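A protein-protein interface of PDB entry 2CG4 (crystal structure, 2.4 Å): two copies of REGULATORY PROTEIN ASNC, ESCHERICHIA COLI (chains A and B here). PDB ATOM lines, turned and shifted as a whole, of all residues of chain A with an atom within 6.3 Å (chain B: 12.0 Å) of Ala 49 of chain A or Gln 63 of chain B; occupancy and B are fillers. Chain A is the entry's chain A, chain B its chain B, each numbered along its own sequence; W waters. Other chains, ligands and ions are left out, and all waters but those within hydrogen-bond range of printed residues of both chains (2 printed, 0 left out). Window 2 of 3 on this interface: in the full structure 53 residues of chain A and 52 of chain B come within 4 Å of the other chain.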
ATOM      1  N   TYR A   4      -4.864  29.471 -19.452  1.00  0.00           N
ATOM      2  CA  TYR A   4      -3.747  30.155 -20.162  1.00  0.00           C
ATOM      3  C   TYR A   4      -4.166  30.589 -21.566  1.00  0.00           C
ATOM      4  O   TYR A   4      -4.562  29.762 -22.390  1.00  0.00           O
ATOM      5  CB  TYR A   4      -2.521  29.239 -20.231  1.00  0.00           C
ATOM      6  CG  TYR A   4      -1.263  29.917 -20.738  1.00  0.00           C
ATOM      7  CD1 TYR A   4      -0.526  30.760 -19.913  1.00  0.00           C
ATOM      8  CD2 TYR A   4      -0.809  29.706 -22.036  1.00  0.00           C
ATOM      9  CE1 TYR A   4       0.623  31.381 -20.368  1.00  0.00           C
ATOM     10  CE2 TYR A   4       0.337  30.321 -22.501  1.00  0.00           C
ATOM     11  CZ  TYR A   4       1.050  31.158 -21.662  1.00  0.00           C
ATOM     12  OH  TYR A   4       2.196  31.778 -22.115  1.00  0.00           O
ATOM     13  N   GLU A  44       7.867  27.014 -22.901  1.00  0.00           N
ATOM     14  CA  GLU A  44       7.962  26.539 -21.523  1.00  0.00           C
ATOM     15  C   GLU A  44       6.713  26.878 -20.714  1.00  0.00           C
ATOM     16  O   GLU A  44       6.307  26.120 -19.835  1.00  0.00           O
ATOM     17  CB  GLU A  44       9.193  27.132 -20.837  1.00  0.00           C
ATOM     18  CG  GLU A  44      10.003  26.131 -20.025  1.00  0.00           C
ATOM     19  CD  GLU A  44       9.260  25.593 -18.812  1.00  0.00           C
ATOM     20  OE1 GLU A  44       9.771  25.756 -17.683  1.00  0.00           O
ATOM     21  OE2 GLU A  44       8.173  24.999 -18.983  1.00  0.00           O
ATOM     22  N   LYS A  45       6.117  28.030 -21.004  1.00  0.00           N
ATOM     23  CA  LYS A  45       4.842  28.391 -20.397  1.00  0.00           C
ATOM     24  C   LYS A  45       3.740  27.428 -20.850  1.00  0.00           C
ATOM     25  O   LYS A  45       2.986  26.912 -20.026  1.00  0.00           O
ATOM     26  CB  LYS A  45       4.476  29.841 -20.727  1.00  0.00           C
ATOM     27  CG  LYS A  45       5.137  30.890 -19.823  1.00  0.00           C
ATOM     28  CD  LYS A  45       5.087  32.269 -20.482  1.00  0.00           C
ATOM     29  CE  LYS A  45       6.016  33.271 -19.806  1.00  0.00           C
ATOM     30  NZ  LYS A  45       6.185  34.517 -20.621  1.00  0.00           N
ATOM     31  N   MET A  46       3.666  27.177 -22.157  1.00  0.00           N
ATOM     32  CA  MET A  46       2.733  26.194 -22.717  1.00  0.00           C
ATOM     33  C   MET A  46       2.913  24.779 -22.161  1.00  0.00           C
ATOM     34  O   MET A  46       1.948  24.033 -22.063  1.00  0.00           O
ATOM     35  CB  MET A  46       2.808  26.181 -24.242  1.00  0.00           C
ATOM     36  CG  MET A  46       2.378  27.485 -24.861  1.00  0.00           C
ATOM     37  SD  MET A  46       2.160  27.413 -26.646  1.00  0.00           S
ATOM     38  CE  MET A  46       3.812  27.803 -27.228  1.00  0.00           C
ATOM     39  N   LYS A  47       4.133  24.413 -21.783  1.00  0.00           N
ATOM     40  CA  LYS A  47       4.348  23.136 -21.102  1.00  0.00           C
ATOM     41  C   LYS A  47       3.734  23.102 -19.701  1.00  0.00           C
ATOM     42  O   LYS A  47       3.047  22.139 -19.355  1.00  0.00           O
ATOM     43  CB  LYS A  47       5.834  22.770 -21.050  1.00  0.00           C
ATOM     44  CG  LYS A  47       6.411  22.338 -22.390  1.00  0.00           C
ATOM     45  CD  LYS A  47       7.829  21.811 -22.244  1.00  0.00           C
ATOM     46  CE  LYS A  47       8.657  22.142 -23.477  1.00  0.00           C
ATOM     47  NZ  LYS A  47      10.019  21.510 -23.453  1.00  0.00           N
ATOM     48  N   GLN A  48       3.974  24.141 -18.899  1.00  0.00           N
ATOM     49  CA  GLN A  48       3.369  24.229 -17.561  1.00  0.00           C
ATOM     50  C   GLN A  48       1.850  24.458 -17.607  1.00  0.00           C
ATOM     51  O   GLN A  48       1.115  23.969 -16.740  1.00  0.00           O
ATOM     52  CB  GLN A  48       4.058  25.306 -16.720  1.00  0.00           C
ATOM     53  N   ALA A  49       1.386  25.190 -18.619  1.00  0.00           N
ATOM     54  CA  ALA A  49      -0.042  25.270 -18.935  1.00  0.00           C
ATOM     55  C   ALA A  49      -0.665  23.899 -19.216  1.00  0.00           C
ATOM     56  O   ALA A  49      -1.852  23.690 -18.979  1.00  0.00           O
ATOM     57  CB  ALA A  49      -0.274  26.205 -20.119  1.00  0.00           C
ATOM     58  N   GLY A  50       0.139  22.969 -19.722  1.00  0.00           N
ATOM     59  CA  GLY A  50      -0.354  21.643 -20.072  1.00  0.00           C
ATOM     60  C   GLY A  50      -0.804  21.564 -21.517  1.00  0.00           C
ATOM     61  O   GLY A  50      -1.352  20.543 -21.945  1.00  0.00           O
ATOM     62  N   ILE A  51      -0.571  22.643 -22.267  1.00  0.00           N
ATOM     63  CA  ILE A  51      -0.930  22.709 -23.683  1.00  0.00           C
ATOM     64  C   ILE A  51      -0.032  21.788 -24.512  1.00  0.00           C
ATOM     65  O   ILE A  51      -0.517  20.921 -25.255  1.00  0.00           O
ATOM     66  CB  ILE A  51      -0.808  24.156 -24.230  1.00  0.00           C
ATOM     67  CG1 ILE A  51      -2.012  25.000 -23.809  1.00  0.00           C
ATOM     68  CG2 ILE A  51      -0.682  24.158 -25.735  1.00  0.00           C
ATOM     69  CD1 ILE A  51      -1.707  26.477 -23.659  1.00  0.00           C
ATOM     70  N   ILE A  52       1.276  22.003 -24.390  1.00  0.00           N
ATOM     71  CA  ILE A  52       2.278  21.112 -24.952  1.00  0.00           C
ATOM     72  C   ILE A  52       2.539  19.979 -23.966  1.00  0.00           C
ATOM     73  O   ILE A  52       2.985  20.226 -22.847  1.00  0.00           O
ATOM     74  CB  ILE A  52       3.587  21.878 -25.238  1.00  0.00           C
ATOM     75  CG1 ILE A  52       3.339  22.977 -26.277  1.00  0.00           C
ATOM     76  CG2 ILE A  52       4.702  20.925 -25.675  1.00  0.00           C
ATOM     77  CD1 ILE A  52       4.607  23.639 -26.790  1.00  0.00           C
ATOM     78  N   ILE B  57       5.673  17.633 -31.399  1.00  0.00           N
ATOM     79  CA  ILE B  57       5.144  17.871 -30.062  1.00  0.00           C
ATOM     80  C   ILE B  57       3.680  17.480 -30.036  1.00  0.00           C
ATOM     81  O   ILE B  57       2.944  17.703 -31.006  1.00  0.00           O
ATOM     82  CB  ILE B  57       5.305  19.345 -29.571  1.00  0.00           C
ATOM     83  CG1 ILE B  57       4.292  20.267 -30.252  1.00  0.00           C
ATOM     84  CG2 ILE B  57       6.738  19.850 -29.767  1.00  0.00           C
ATOM     85  CD1 ILE B  57       3.605  21.221 -29.300  1.00  0.00           C
ATOM     86  N   ASP B  58       3.263  16.880 -28.925  1.00  0.00           N
ATOM     87  CA  ASP B  58       1.856  16.601 -28.707  1.00  0.00           C
ATOM     88  C   ASP B  58       1.176  17.753 -27.984  1.00  0.00           C
ATOM     89  O   ASP B  58       1.768  18.424 -27.141  1.00  0.00           O
ATOM     90  CB  ASP B  58       1.669  15.284 -27.955  1.00  0.00           C
ATOM     91  CG  ASP B  58       2.054  14.072 -28.792  1.00  0.00           C
ATOM     92  OD1 ASP B  58       2.475  13.057 -28.206  1.00  0.00           O
ATOM     93  OD2 ASP B  58       1.944  14.134 -30.036  1.00  0.00           O
ATOM     94  N   VAL B  59      -0.076  17.983 -28.341  1.00  0.00           N
ATOM     95  CA  VAL B  59      -0.818  19.128 -27.863  1.00  0.00           C
ATOM     96  C   VAL B  59      -2.090  18.618 -27.200  1.00  0.00           C
ATOM     97  O   VAL B  59      -2.638  17.592 -27.602  1.00  0.00           O
ATOM     98  CB  VAL B  59      -1.147  20.087 -29.033  1.00  0.00           C
ATOM     99  CG1 VAL B  59      -2.570  20.600 -28.938  1.00  0.00           C
ATOM    100  CG2 VAL B  59      -0.150  21.242 -29.081  1.00  0.00           C
ATOM    101  N   SER B  60      -2.548  19.315 -26.173  1.00  0.00           N
ATOM    102  CA  SER B  60      -3.817  18.973 -25.549  1.00  0.00           C
ATOM    103  C   SER B  60      -4.909  19.925 -26.006  1.00  0.00           C
ATOM    104  O   SER B  60      -4.850  21.112 -25.702  1.00  0.00           O
ATOM    105  CB  SER B  60      -3.700  19.005 -24.023  1.00  0.00           C
ATOM    106  OG  SER B  60      -4.954  19.299 -23.439  1.00  0.00           O
ATOM    107  N   PRO B  61      -5.909  19.407 -26.739  1.00  0.00           N
ATOM    108  CA  PRO B  61      -7.001  20.244 -27.229  1.00  0.00           C
ATOM    109  C   PRO B  61      -7.789  20.884 -26.088  1.00  0.00           C
ATOM    110  O   PRO B  61      -8.209  22.031 -26.199  1.00  0.00           O
ATOM    111  CB  PRO B  61      -7.891  19.254 -27.997  1.00  0.00           C
ATOM    112  CG  PRO B  61      -6.998  18.103 -28.314  1.00  0.00           C
ATOM    113  CD  PRO B  61      -6.066  18.001 -27.151  1.00  0.00           C
ATOM    114  N   LYS B  62      -7.989  20.135 -25.008  1.00  0.00           N
ATOM    115  CA  LYS B  62      -8.720  20.621 -23.845  1.00  0.00           C
ATOM    116  C   LYS B  62      -8.120  21.926 -23.318  1.00  0.00           C
ATOM    117  O   LYS B  62      -8.839  22.913 -23.103  1.00  0.00           O
ATOM    118  CB  LYS B  62      -8.717  19.558 -22.747  1.00  0.00           C
ATOM    119  CG  LYS B  62      -9.684  19.837 -21.613  1.00  0.00           C
ATOM    120  CD  LYS B  62      -9.787  18.642 -20.667  1.00  0.00           C
ATOM    121  CE  LYS B  62      -8.691  18.660 -19.602  1.00  0.00           C
ATOM    122  NZ  LYS B  62      -9.036  17.807 -18.420  1.00  0.00           N
ATOM    123  N   GLN B  63      -6.802  21.924 -23.127  1.00  0.00           N
ATOM    124  CA  GLN B  63      -6.079  23.090 -22.637  1.00  0.00           C
ATOM    125  C   GLN B  63      -6.100  24.252 -23.629  1.00  0.00           C
ATOM    126  O   GLN B  63      -5.884  25.412 -23.253  1.00  0.00           O
ATOM    127  CB  GLN B  63      -4.643  22.708 -22.301  1.00  0.00           C
ATOM    128  CG  GLN B  63      -4.329  22.727 -20.814  1.00  0.00           C
ATOM    129  CD  GLN B  63      -5.306  21.933 -19.980  1.00  0.00           C
ATOM    130  OE1 GLN B  63      -4.910  21.069 -19.203  1.00  0.00           O
ATOM    131  NE2 GLN B  63      -6.591  22.223 -20.131  1.00  0.00           N
ATOM    132  N   LEU B  64      -6.364  23.939 -24.894  1.00  0.00           N
ATOM    133  CA  LEU B  64      -6.524  24.964 -25.920  1.00  0.00           C
ATOM    134  C   LEU B  64      -7.994  25.337 -26.099  1.00  0.00           C
ATOM    135  O   LEU B  64      -8.355  26.055 -27.039  1.00  0.00           O
ATOM    136  CB  LEU B  64      -5.925  24.493 -27.246  1.00  0.00           C
ATOM    137  CG  LEU B  64      -4.397  24.522 -27.367  1.00  0.00           C
ATOM    138  CD1 LEU B  64      -3.933  23.545 -28.423  1.00  0.00           C
ATOM    139  CD2 LEU B  64      -3.901  25.933 -27.690  1.00  0.00           C
ATOM    140  N   GLY B  65      -8.834  24.844 -25.191  1.00  0.00           N
ATOM    141  CA  GLY B  65     -10.219  25.298 -25.091  1.00  0.00           C
ATOM    142  C   GLY B  65     -11.213  24.511 -25.930  1.00  0.00           C
ATOM    143  O   GLY B  65     -12.343  24.957 -26.147  1.00  0.00           O
ATOM    144  N   TYR B  66     -10.801  23.341 -26.409  1.00  0.00           N
ATOM    145  CA  TYR B  66     -11.719  22.439 -27.106  1.00  0.00           C
ATOM    146  C   TYR B  66     -12.489  21.571 -26.113  1.00  0.00           C
ATOM    147  O   TYR B  66     -12.098  20.442 -25.811  1.00  0.00           O
ATOM    148  CB  TYR B  66     -10.972  21.580 -28.127  1.00  0.00           C
ATOM    149  CG  TYR B  66     -10.359  22.378 -29.259  1.00  0.00           C
ATOM    150  CD1 TYR B  66      -9.074  22.914 -29.154  1.00  0.00           C
ATOM    151  CD2 TYR B  66     -11.068  22.605 -30.434  1.00  0.00           C
ATOM    152  CE1 TYR B  66      -8.516  23.641 -30.195  1.00  0.00           C
ATOM    153  CE2 TYR B  66     -10.521  23.331 -31.476  1.00  0.00           C
ATOM    154  CZ  TYR B  66      -9.250  23.845 -31.353  1.00  0.00           C
ATOM    155  OH  TYR B  66      -8.724  24.564 -32.403  1.00  0.00           O
ATOM    156  N   ASP B  67     -13.587  22.127 -25.612  1.00  0.00           N
ATOM    157  CA  ASP B  67     -14.405  21.493 -24.595  1.00  0.00           C
ATOM    158  C   ASP B  67     -15.419  20.517 -25.188  1.00  0.00           C
ATOM    159  O   ASP B  67     -16.021  19.720 -24.467  1.00  0.00           O
ATOM    160  CB  ASP B  67     -15.139  22.568 -23.788  1.00  0.00           C
ATOM    161  CG  ASP B  67     -14.202  23.379 -22.916  1.00  0.00           C
ATOM    162  OD1 ASP B  67     -13.171  22.827 -22.469  1.00  0.00           O
ATOM    163  OD2 ASP B  67     -14.501  24.569 -22.672  1.00  0.00           O
ATOM    164  N   VAL B  68     -15.627  20.594 -26.498  1.00  0.00           N
ATOM    165  CA  VAL B  68     -16.603  19.725 -27.146  1.00  0.00           C
ATOM    166  C   VAL B  68     -15.968  18.867 -28.244  1.00  0.00           C
ATOM    167  O   VAL B  68     -15.881  19.270 -29.410  1.00  0.00           O
ATOM    168  CB  VAL B  68     -17.811  20.514 -27.684  1.00  0.00           C
ATOM    169  CG1 VAL B  68     -18.798  19.573 -28.316  1.00  0.00           C
ATOM    170  CG2 VAL B  68     -18.477  21.278 -26.561  1.00  0.00           C
ATOM    171  N   GLY B  69     -15.505  17.693 -27.844  1.00  0.00           N
ATOM    172  CA  GLY B  69     -15.171  16.639 -28.775  1.00  0.00           C
ATOM    173  C   GLY B  69     -16.396  15.813 -29.104  1.00  0.00           C
ATOM    174  O   GLY B  69     -17.240  15.546 -28.246  1.00  0.00           O
ATOM    175  N   MET B 112     -13.615  18.268 -33.578  1.00  0.00           N
ATOM    176  CA  MET B 112     -13.172  18.912 -32.348  1.00  0.00           C
ATOM    177  C   MET B 112     -13.557  20.385 -32.371  1.00  0.00           C
ATOM    178  O   MET B 112     -13.237  21.103 -33.313  1.00  0.00           O
ATOM    179  CB  MET B 112     -11.665  18.744 -32.164  1.00  0.00           C
ATOM    180  CG  MET B 112     -11.212  17.306 -31.979  1.00  0.00           C
ATOM    181  SD  MET B 112     -11.649  16.609 -30.381  1.00  0.00           S
ATOM    182  CE  MET B 112     -11.040  17.874 -29.268  1.00  0.00           C
ATOM    183  N   CYS B 113     -14.274  20.814 -31.334  1.00  0.00           N
ATOM    184  CA  CYS B 113     -14.939  22.119 -31.309  1.00  0.00           C
ATOM    185  C   CYS B 113     -14.723  22.778 -29.956  1.00  0.00           C
ATOM    186  O   CYS B 113     -14.451  22.095 -28.966  1.00  0.00           O
ATOM    187  CB  CYS B 113     -16.439  21.953 -31.558  1.00  0.00           C
ATOM    188  SG  CYS B 113     -16.913  21.890 -33.290  1.00  0.00           S
ATOM    189  N   ARG B 114     -14.862  24.098 -29.896  1.00  0.00           N
ATOM    190  CA  ARG B 114     -14.657  24.807 -28.634  1.00  0.00           C
ATOM    191  C   ARG B 114     -15.896  24.833 -27.745  1.00  0.00           C
ATOM    192  O   ARG B 114     -15.794  24.673 -26.524  1.00  0.00           O
ATOM    193  CB  ARG B 114     -14.140  26.221 -28.875  1.00  0.00           C
ATOM    194  CG  ARG B 114     -12.647  26.294 -29.147  1.00  0.00           C
ATOM    195  CD  ARG B 114     -12.270  27.666 -29.683  1.00  0.00           C
ATOM    196  NE  ARG B 114     -11.268  27.581 -30.743  1.00  0.00           N
ATOM    197  CZ  ARG B 114      -9.958  27.494 -30.529  1.00  0.00           C
ATOM    198  NH1 ARG B 114      -9.493  27.469 -29.287  1.00  0.00           N
ATOM    199  NH2 ARG B 114      -9.115  27.423 -31.553  1.00  0.00           N
ATOM    200  N   SER B 115     -17.065  25.029 -28.351  1.00  0.00           N
ATOM    201  CA  SER B 115     -18.316  25.024 -27.593  1.00  0.00           C
ATOM    202  C   SER B 115     -19.439  24.326 -28.355  1.00  0.00           C
ATOM    203  O   SER B 115     -19.305  24.041 -29.546  1.00  0.00           O
ATOM    204  CB  SER B 115     -18.734  26.455 -27.256  1.00  0.00           C
ATOM    205  OG  SER B 115     -18.865  27.230 -28.436  1.00  0.00           O
ATOM    206  N   ASN B 144     -13.171  11.772 -21.566  1.00  0.00           N
ATOM    207  CA  ASN B 144     -12.214  11.029 -22.368  1.00  0.00           C
ATOM    208  C   ASN B 144     -11.035  10.525 -21.535  1.00  0.00           C
ATOM    209  O   ASN B 144      -9.916  11.006 -21.694  1.00  0.00           O
ATOM    210  CB  ASN B 144     -11.692  11.912 -23.504  1.00  0.00           C
ATOM    211  CG  ASN B 144     -10.525  11.285 -24.236  1.00  0.00           C
ATOM    212  OD1 ASN B 144     -10.532  10.091 -24.549  1.00  0.00           O
ATOM    213  ND2 ASN B 144      -9.519  12.083 -24.514  1.00  0.00           N
ATOM    214  N   MET B 147      -6.600   8.088 -23.368  1.00  0.00           N
ATOM    215  CA  MET B 147      -6.065   8.455 -24.670  1.00  0.00           C
ATOM    216  C   MET B 147      -4.585   8.093 -24.714  1.00  0.00           C
ATOM    217  O   MET B 147      -3.770   8.664 -23.983  1.00  0.00           O
ATOM    218  CB  MET B 147      -6.249   9.949 -24.938  1.00  0.00           C
ATOM    219  CG  MET B 147      -7.537  10.293 -25.681  1.00  0.00           C
ATOM    220  SD  MET B 147      -7.448  10.144 -27.482  1.00  0.00           S
ATOM    221  CE  MET B 147      -5.684   9.972 -27.740  1.00  0.00           C
HETATM  222  O   HOH W   1      -5.949  28.270 -24.164  1.00  0.00           O
HETATM  223  O   HOH W   2      -4.407  24.329 -18.165  1.00  0.00           O
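Among the printed residues, merely in contact across the chains: Ile 51 of chain A with Val 59 of chain B, Ala 49 of chain A with Gln 63 of chain B, Gly 50 of chain A with Ser 60 of chain B, Ile 52 of chain A with Asp 58 of chain B, Ile 52 of chain A with Ile 57 of chain B, Gly 50 of chain A with Gln 63 of chain B, Ile 51 of chain A with Gln 63 of chain B and Ile 51 of chain A with Asp 58 of chain B.
N of Ser 60 of chain B lies within hydrogen-bond range of O of Ile 51 of chain A, 2.7 Å away.
No residue of chain B comes within 4 Å of Tyr 4 of chain A. Glu 44 of chain A touches none of the printed residues of chain B. Gln 48 of chain A touches none of the printed residues of chain B. Of chain B, only Gln 63 (3.2 Å) comes within 4 Å of Ala 49 of chain A. Gly 50 of chain A touches two residues of chain B. Printed residues of chain B within 4 Å of Ile 52 of chain A: Ile 57 (3.5 Å) and Asp 58 (3.5 Å). Of the printed residues of chain A, Ser 60 of chain B touches Gly 50 (3.5 Å) and Ile 51 (2.7 Å). Gln 63 of chain B touches three residues of chain A. The nearest residue of chain A that does not touch Gln 63 of chain B is Tyr 4 of chain A (4.6 Å). The nearest printed residue of chain B that does not touch Ile 52 of chain A is Val 59 of chain B (4.7 Å).
The backbone carbonyl oxygen (O) of Met 46 of chain A lies within hydrogen-bond range of the backbone NH (N) of Ile 51 of chain A (2.9 Å). O of Met 46 of chain A is in hydrogen-bond range of N of Ile 52 of chain A, at 3.2 Å. The backbone NH (N) of Gln 63 of chain B sits at hydrogen-bond distance from the side-chain hydroxyl (OG) of Ser 60 of chain B, at 3.2 Å.
Of the 19 printed residues of chain B, 5 touch a printed residue of chain A. Hydrophobic or aromatic side chains of chain B within 4 Å of the printed part of chain A: Ile 57 and Val 59. Of the 10 printed residues of chain A, 4 touch a printed residue of chain B. Printed residues of chain A that touch a printed residue of chain B: Ala 49, Gly 50, Ile 51 and Ile 52. Among the printed residues, 9 pairs touch across the chains.
Water W1 bridges O of Tyr 4 of chain A and O of Gln 63 of chain B. Water W2 lies within hydrogen-bond range of the backbone carbonyl oxygen (O) of Ala 49 of chain A (2.8 Å) and the side-chain amide oxygen (OE1) of Gln 63 of chain B (3.5 Å).
No position is printed for both chains.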
